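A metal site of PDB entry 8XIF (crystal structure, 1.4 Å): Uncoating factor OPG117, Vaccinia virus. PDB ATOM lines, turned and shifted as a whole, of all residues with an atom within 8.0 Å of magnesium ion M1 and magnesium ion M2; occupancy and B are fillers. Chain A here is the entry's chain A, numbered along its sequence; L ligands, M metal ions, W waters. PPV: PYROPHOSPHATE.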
ATOM      1  N   MET A  69      -3.312  20.617 -22.810  1.00  0.00           N
ATOM      2  CA  MET A  69      -3.733  19.242 -23.066  1.00  0.00           C
ATOM      3  C   MET A  69      -2.575  18.309 -22.724  1.00  0.00           C
ATOM      4  O   MET A  69      -1.393  18.645 -22.908  1.00  0.00           O
ATOM      5  CB  MET A  69      -4.086  18.937 -24.543  1.00  0.00           C
ATOM      6  CG  MET A  69      -5.479  19.346 -24.965  1.00  0.00           C
ATOM      7  SD  MET A  69      -5.436  21.077 -25.446  1.00  0.00           S
ATOM      8  CE  MET A  69      -7.171  21.368 -25.811  1.00  0.00           C
ATOM      9  N   ASP A  70      -2.943  17.151 -22.217  1.00  0.00           N
ATOM     10  CA  ASP A  70      -2.042  16.042 -21.922  1.00  0.00           C
ATOM     11  C   ASP A  70      -2.337  15.000 -22.981  1.00  0.00           C
ATOM     12  O   ASP A  70      -3.412  14.412 -22.968  1.00  0.00           O
ATOM     13  CB  ASP A  70      -2.393  15.527 -20.518  1.00  0.00           C
ATOM     14  CG  ASP A  70      -1.727  14.212 -20.177  1.00  0.00           C
ATOM     15  OD1 ASP A  70      -0.585  13.961 -20.631  1.00  0.00           O
ATOM     16  OD2 ASP A  70      -2.339  13.427 -19.425  1.00  0.00           O
ATOM     17  N   VAL A  71      -1.387  14.750 -23.881  1.00  0.00           N
ATOM     18  CA  VAL A  71      -1.600  13.850 -25.016  1.00  0.00           C
ATOM     19  C   VAL A  71      -0.801  12.569 -24.772  1.00  0.00           C
ATOM     20  O   VAL A  71       0.433  12.611 -24.632  1.00  0.00           O
ATOM     21  CB  VAL A  71      -1.238  14.512 -26.352  1.00  0.00           C
ATOM     22  CG1 VAL A  71      -1.351  13.496 -27.521  1.00  0.00           C
ATOM     23  CG2 VAL A  71      -2.144  15.751 -26.596  1.00  0.00           C
ATOM     24  N   ASP A  72      -1.507  11.438 -24.746  1.00  0.00           N
ATOM     25  CA  ASP A  72      -0.985  10.150 -24.279  1.00  0.00           C
ATOM     26  C   ASP A  72      -1.155   9.109 -25.374  1.00  0.00           C
ATOM     27  O   ASP A  72      -2.028   8.248 -25.288  1.00  0.00           O
ATOM     28  CB  ASP A  72      -1.731   9.662 -23.023  1.00  0.00           C
ATOM     29  CG  ASP A  72      -1.485  10.550 -21.810  1.00  0.00           C
ATOM     30  OD1 ASP A  72      -0.414  11.224 -21.718  1.00  0.00           O
ATOM     31  OD2 ASP A  72      -2.399  10.624 -20.949  1.00  0.00           O
ATOM     32  N   LEU A  73      -0.343   9.177 -26.428  1.00  0.00           N
ATOM     33  CA  LEU A  73      -0.426   8.169 -27.478  1.00  0.00           C
ATOM     34  C   LEU A  73       0.553   7.035 -27.173  1.00  0.00           C
ATOM     35  O   LEU A  73       1.772   7.241 -27.159  1.00  0.00           O
ATOM     36  CB  LEU A  73      -0.146   8.765 -28.857  1.00  0.00           C
ATOM     37  CG  LEU A  73      -0.102   7.752 -30.007  1.00  0.00           C
ATOM     38  CD1 LEU A  73      -1.402   6.957 -30.136  1.00  0.00           C
ATOM     39  CD2 LEU A  73       0.225   8.469 -31.336  1.00  0.00           C
ATOM     40  N   THR A 123       6.029  19.978 -25.054  1.00  0.00           N
ATOM     41  CA  THR A 123       7.090  19.143 -24.535  1.00  0.00           C
ATOM     42  C   THR A 123       7.244  17.910 -25.413  1.00  0.00           C
ATOM     43  O   THR A 123       6.475  17.695 -26.356  1.00  0.00           O
ATOM     44  CB  THR A 123       6.799  18.677 -23.118  1.00  0.00           C
ATOM     45  OG1 THR A 123       5.655  17.798 -23.130  1.00  0.00           O
ATOM     46  CG2 THR A 123       6.562  19.820 -22.187  1.00  0.00           C
ATOM     47  N   SER A 125       8.066  13.727 -24.363  1.00  0.00           N
ATOM     48  CA  SER A 125       8.537  12.715 -23.444  1.00  0.00           C
ATOM     49  C   SER A 125       9.727  11.988 -24.060  1.00  0.00           C
ATOM     50  O   SER A 125       9.749  11.713 -25.256  1.00  0.00           O
ATOM     51  CB  SER A 125       7.424  11.690 -23.173  1.00  0.00           C
ATOM     52  OG  SER A 125       7.980  10.584 -22.456  1.00  0.00           O
ATOM     53  N   LYS A 130       6.593   5.690 -27.042  1.00  0.00           N
ATOM     54  CA  LYS A 130       5.275   6.308 -27.113  1.00  0.00           C
ATOM     55  C   LYS A 130       5.428   7.709 -27.676  1.00  0.00           C
ATOM     56  O   LYS A 130       6.539   8.147 -27.987  1.00  0.00           O
ATOM     57  CB  LYS A 130       4.528   6.181 -25.785  1.00  0.00           C
ATOM     58  CG  LYS A 130       5.132   6.922 -24.664  1.00  0.00           C
ATOM     59  CD  LYS A 130       4.460   6.500 -23.368  1.00  0.00           C
ATOM     60  CE  LYS A 130       4.761   7.476 -22.252  1.00  0.00           C
ATOM     61  NZ  LYS A 130       3.949   7.205 -21.024  1.00  0.00           N
ATOM     62  N   THR A 131       4.295   8.365 -27.888  1.00  0.00           N
ATOM     63  CA  THR A 131       4.238   9.728 -28.384  1.00  0.00           C
ATOM     64  C   THR A 131       3.444  10.501 -27.340  1.00  0.00           C
ATOM     65  O   THR A 131       2.220  10.603 -27.381  1.00  0.00           O
ATOM     66  CB  THR A 131       3.599   9.793 -29.784  1.00  0.00           C
ATOM     67  OG1 THR A 131       4.273   8.887 -30.649  1.00  0.00           O
ATOM     68  CG2 THR A 131       3.745  11.226 -30.339  1.00  0.00           C
ATOM     69  N   SER A 132       4.163  11.059 -26.376  1.00  0.00           N
ATOM     70  CA  SER A 132       3.548  11.684 -25.227  1.00  0.00           C
ATOM     71  C   SER A 132       4.050  13.117 -25.143  1.00  0.00           C
ATOM     72  O   SER A 132       5.253  13.365 -25.286  1.00  0.00           O
ATOM     73  CB  SER A 132       3.969  10.933 -23.974  1.00  0.00           C
ATOM     74  OG  SER A 132       3.814  11.784 -22.846  1.00  0.00           O
ATOM     75  N   PHE A 133       3.125  14.056 -24.918  1.00  0.00           N
ATOM     76  CA  PHE A 133       3.542  15.439 -24.782  1.00  0.00           C
ATOM     77  C   PHE A 133       2.483  16.194 -24.016  1.00  0.00           C
ATOM     78  O   PHE A 133       1.339  15.764 -23.891  1.00  0.00           O
ATOM     79  CB  PHE A 133       3.841  16.093 -26.154  1.00  0.00           C
ATOM     80  CG  PHE A 133       2.644  16.195 -27.077  1.00  0.00           C
ATOM     81  CD1 PHE A 133       1.780  17.274 -26.990  1.00  0.00           C
ATOM     82  CD2 PHE A 133       2.430  15.246 -28.073  1.00  0.00           C
ATOM     83  CE1 PHE A 133       0.665  17.398 -27.860  1.00  0.00           C
ATOM     84  CE2 PHE A 133       1.329  15.379 -28.947  1.00  0.00           C
ATOM     85  CZ  PHE A 133       0.462  16.458 -28.851  1.00  0.00           C
ATOM     86  N   HIS A 134       2.899  17.328 -23.459  1.00  0.00           N
ATOM     87  CA  HIS A 134       2.004  18.345 -22.942  1.00  0.00           C
ATOM     88  C   HIS A 134       2.031  19.557 -23.856  1.00  0.00           C
ATOM     89  O   HIS A 134       3.094  19.962 -24.337  1.00  0.00           O
ATOM     90  CB  HIS A 134       2.370  18.783 -21.515  1.00  0.00           C
ATOM     91  CG  HIS A 134       2.372  17.654 -20.526  1.00  0.00           C
ATOM     92  ND1 HIS A 134       3.199  17.646 -19.428  1.00  0.00           N
ATOM     93  CD2 HIS A 134       1.757  16.439 -20.548  1.00  0.00           C
ATOM     94  CE1 HIS A 134       3.010  16.518 -18.752  1.00  0.00           C
ATOM     95  NE2 HIS A 134       2.147  15.763 -19.428  1.00  0.00           N
ATOM     96  N   SER A 168      -5.765  10.852 -28.663  1.00  0.00           N
ATOM     97  CA  SER A 168      -5.052  10.530 -27.436  1.00  0.00           C
ATOM     98  C   SER A 168      -5.118  11.625 -26.382  1.00  0.00           C
ATOM     99  O   SER A 168      -4.395  11.540 -25.390  1.00  0.00           O
ATOM    100  CB  SER A 168      -3.595  10.144 -27.731  1.00  0.00           C
ATOM    101  OG  SER A 168      -3.594   9.084 -28.661  1.00  0.00           O
ATOM    102  N   ILE A 169      -5.940  12.663 -26.580  1.00  0.00           N
ATOM    103  CA  ILE A 169      -6.140  13.682 -25.557  1.00  0.00           C
ATOM    104  C   ILE A 169      -6.688  13.017 -24.307  1.00  0.00           C
ATOM    105  O   ILE A 169      -7.679  12.267 -24.366  1.00  0.00           O
ATOM    106  CB  ILE A 169      -7.090  14.772 -26.066  1.00  0.00           C
ATOM    107  CG1 ILE A 169      -6.413  15.569 -27.190  1.00  0.00           C
ATOM    108  CG2 ILE A 169      -7.488  15.714 -24.917  1.00  0.00           C
ATOM    109  CD1 ILE A 169      -7.415  16.461 -27.965  1.00  0.00           C
ATOM    110  N   ASP A 170      -6.053  13.284 -23.170  1.00  0.00           N
ATOM    111  CA  ASP A 170      -6.494  12.682 -21.909  1.00  0.00           C
ATOM    112  C   ASP A 170      -7.409  13.704 -21.261  1.00  0.00           C
ATOM    113  O   ASP A 170      -6.955  14.698 -20.676  1.00  0.00           O
ATOM    114  CB  ASP A 170      -5.272  12.376 -21.039  1.00  0.00           C
ATOM    115  CG  ASP A 170      -5.649  11.788 -19.688  1.00  0.00           C
ATOM    116  OD1 ASP A 170      -6.859  11.613 -19.408  1.00  0.00           O
ATOM    117  OD2 ASP A 170      -4.716  11.416 -18.922  1.00  0.00           O
ATOM    118  N   THR A 171      -8.722  13.492 -21.399  1.00  0.00           N
ATOM    119  CA  THR A 171      -9.641  14.468 -20.816  1.00  0.00           C
ATOM    120  C   THR A 171      -9.812  14.324 -19.321  1.00  0.00           C
ATOM    121  O   THR A 171     -10.454  15.200 -18.712  1.00  0.00           O
ATOM    122  CB  THR A 171     -11.000  14.431 -21.513  1.00  0.00           C
ATOM    123  OG1 THR A 171     -11.646  13.185 -21.257  1.00  0.00           O
ATOM    124  CG2 THR A 171     -10.867  14.674 -23.002  1.00  0.00           C
ATOM    125  N   ALA A 172      -9.238  13.291 -18.695  1.00  0.00           N
ATOM    126  CA  ALA A 172      -9.402  13.138 -17.251  1.00  0.00           C
ATOM    127  C   ALA A 172      -8.690  14.248 -16.487  1.00  0.00           C
ATOM    128  O   ALA A 172      -8.982  14.469 -15.302  1.00  0.00           O
ATOM    129  CB  ALA A 172      -8.892  11.780 -16.788  1.00  0.00           C
ATOM    130  N   VAL A 173      -7.786  14.987 -17.142  1.00  0.00           N
ATOM    131  CA  VAL A 173      -7.058  16.038 -16.448  1.00  0.00           C
ATOM    132  C   VAL A 173      -7.928  17.249 -16.170  1.00  0.00           C
ATOM    133  O   VAL A 173      -7.502  18.124 -15.412  1.00  0.00           O
ATOM    134  CB  VAL A 173      -5.794  16.468 -17.225  1.00  0.00           C
ATOM    135  CG1 VAL A 173      -4.901  15.242 -17.483  1.00  0.00           C
ATOM    136  CG2 VAL A 173      -6.120  17.186 -18.536  1.00  0.00           C
ATOM    137  N   THR A 179      -3.484  18.216 -11.685  1.00  0.00           N
ATOM    138  CA  THR A 179      -2.040  18.425 -11.710  1.00  0.00           C
ATOM    139  C   THR A 179      -1.500  18.227 -13.119  1.00  0.00           C
ATOM    140  O   THR A 179      -2.063  17.490 -13.933  1.00  0.00           O
ATOM    141  CB  THR A 179      -1.328  17.469 -10.738  1.00  0.00           C
ATOM    142  OG1 THR A 179      -1.558  16.133 -11.176  1.00  0.00           O
ATOM    143  CG2 THR A 179      -1.803  17.665  -9.302  1.00  0.00           C
ATOM    144  N   LEU A 180      -0.367  18.893 -13.401  1.00  0.00           N
ATOM    145  CA  LEU A 180       0.391  18.644 -14.614  1.00  0.00           C
ATOM    146  C   LEU A 180       1.850  18.530 -14.210  1.00  0.00           C
ATOM    147  O   LEU A 180       2.403  19.454 -13.606  1.00  0.00           O
ATOM    148  CB  LEU A 180       0.190  19.769 -15.630  1.00  0.00           C
ATOM    149  CG  LEU A 180       0.802  19.546 -17.010  1.00  0.00           C
ATOM    150  CD1 LEU A 180       0.044  18.453 -17.760  1.00  0.00           C
ATOM    151  CD2 LEU A 180       0.799  20.866 -17.796  1.00  0.00           C
ATOM    152  N   ARG A 181       2.471  17.406 -14.534  1.00  0.00           N
ATOM    153  CA  ARG A 181       3.851  17.204 -14.140  1.00  0.00           C
ATOM    154  C   ARG A 181       4.739  18.288 -14.750  1.00  0.00           C
ATOM    155  O   ARG A 181       4.635  18.614 -15.936  1.00  0.00           O
ATOM    156  CB  ARG A 181       4.279  15.817 -14.604  1.00  0.00           C
ATOM    157  CG  ARG A 181       5.769  15.511 -14.316  1.00  0.00           C
ATOM    158  CD  ARG A 181       6.088  14.042 -14.468  1.00  0.00           C
ATOM    159  NE  ARG A 181       5.805  13.472 -15.785  1.00  0.00           N
ATOM    160  CZ  ARG A 181       6.658  12.727 -16.472  1.00  0.00           C
ATOM    161  NH1 ARG A 181       7.942  12.637 -16.138  1.00  0.00           N
ATOM    162  NH2 ARG A 181       6.208  12.014 -17.499  1.00  0.00           N
ATOM    163  N   LYS A 187       8.116  11.288 -12.911  1.00  0.00           N
ATOM    164  CA  LYS A 187       6.779  10.979 -12.412  1.00  0.00           C
ATOM    165  C   LYS A 187       6.811  10.299 -11.058  1.00  0.00           C
ATOM    166  O   LYS A 187       5.961  10.554 -10.183  1.00  0.00           O
ATOM    167  CB  LYS A 187       6.032  10.125 -13.450  1.00  0.00           C
ATOM    168  CG  LYS A 187       4.729   9.499 -12.999  1.00  0.00           C
ATOM    169  CD  LYS A 187       3.641  10.531 -12.840  1.00  0.00           C
ATOM    170  CE  LYS A 187       3.300  11.181 -14.178  1.00  0.00           C
ATOM    171  NZ  LYS A 187       2.462  12.393 -14.006  1.00  0.00           N
ATOM    172  N   HIS A 195       9.788  14.737 -19.550  1.00  0.00           N
ATOM    173  CA  HIS A 195       9.500  15.580 -20.706  1.00  0.00           C
ATOM    174  C   HIS A 195      10.578  16.642 -20.819  1.00  0.00           C
ATOM    175  O   HIS A 195      10.984  17.241 -19.820  1.00  0.00           O
ATOM    176  CB  HIS A 195       8.163  16.278 -20.527  1.00  0.00           C
ATOM    177  CG  HIS A 195       6.998  15.369 -20.665  1.00  0.00           C
ATOM    178  ND1 HIS A 195       5.878  15.700 -21.398  1.00  0.00           N
ATOM    179  CD2 HIS A 195       6.770  14.127 -20.166  1.00  0.00           C
ATOM    180  CE1 HIS A 195       5.031  14.695 -21.365  1.00  0.00           C
ATOM    181  NE2 HIS A 195       5.528  13.739 -20.619  1.00  0.00           N
HETATM  182  O11 PPV L   1       1.370  11.593 -16.908  1.00  0.00           O
HETATM  183  P1  PPV L   1       2.284  12.517 -17.636  1.00  0.00           P
HETATM  184  O21 PPV L   1       3.056  13.446 -16.728  1.00  0.00           O
HETATM  185  O31 PPV L   1       1.626  13.211 -18.789  1.00  0.00           O
HETATM  186  OPP PPV L   1       3.421  11.599 -18.293  1.00  0.00           O
HETATM  187  P2  PPV L   1       3.380  10.597 -19.553  1.00  0.00           P
HETATM  188  O12 PPV L   1       3.554   9.239 -18.966  1.00  0.00           O
HETATM  189  O22 PPV L   1       2.030  10.759 -20.204  1.00  0.00           O
HETATM  190  O32 PPV L   1       4.505  11.018 -20.451  1.00  0.00           O
HETATM  191 MG    MG M   1      -2.620  11.373 -18.974  1.00  0.00          MG
HETATM  192 MG    MG M   2       0.627  12.283 -20.380  1.00  0.00          MG
HETATM  193  O   HOH W   1      -2.604  11.800 -16.901  1.00  0.00           O
HETATM  194  O   HOH W   2       1.733  13.177 -21.979  1.00  0.00           O
HETATM  195  O   HOH W   3      -2.724   9.316 -18.311  1.00  0.00           O
HETATM  196  O   HOH W   4      -0.485  11.119 -18.847  1.00  0.00           O
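Water W2 lies within hydrogen-bond range of the side-chain hydroxyl (OG) of Ser 132, the backbone carbonyl oxygen (O) of Val 71 and the backbone carbonyl oxygen (O) of Phe 133.
Magnesium ion M1 is bound by OD2 of Asp 170 (2.1 Å), water W1 (2.1 Å), OD2 of Asp 70 (2.1 Å), OD2 of Asp 72 (2.1 Å), water W4 (2.2 Å) and water W3 (2.2 Å).
Of the 23 residues printed, 3 come within 4 Å of magnesium ion M1. The nearest printed residue that does not touch magnesium ion M1 is Val 173 (4.7 Å).
Magnesium ion M2 is bound by OD1 of Asp 72 (2.0 Å), O22 of the ligand (2.1 Å), OD1 of Asp 70 (2.1 Å), O31 of the ligand (2.1 Å), water W2 (2.1 Å) and water W4 (2.2 Å). Magnesium ion M2 has six donor atoms within binding distance.
NE2 of His 134 touches magnesium ion M2, at 3.9 Å. The nearest printed residue that does not touch magnesium ion M2 is Ser 132 (4.1 Å).
The backbone NH of Asp 72 lies within hydrogen-bond range of the backbone carbonyl oxygen of Ser 168, at 3.0 Å. The side-chain carboxylate of Asp 70 sits close to a ring nitrogen (NE2) of His 134 (3.5 Å). The side-chain carboxylate (OD1) of Asp 170 lies within hydrogen-bond range of the backbone NH (N) of Ala 172. N of His 134 lies within hydrogen-bond range of OG1 of Thr 123.
A ring nitrogen (NE2) of His 134 lies close to an oxygen (O31) of the ligand. An oxygen (O32) of the ligand lies within hydrogen-bond range of the side-chain hydroxyl (OG) of Ser 132 (2.6 Å). NE2 of His 195 sits at hydrogen-bond distance from O32 of the ligand (2.9 Å). O12 of the ligand is in salt-bridge range of NZ of Lys 130 (2.9 Å). An oxygen (O21) of the ligand is in salt-bridge range of the guanidinium group (NE) of Arg 181 (2.9 Å). NZ of Lys 187 lies within salt-bridge range of O21 of the ligand (3.0 Å).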
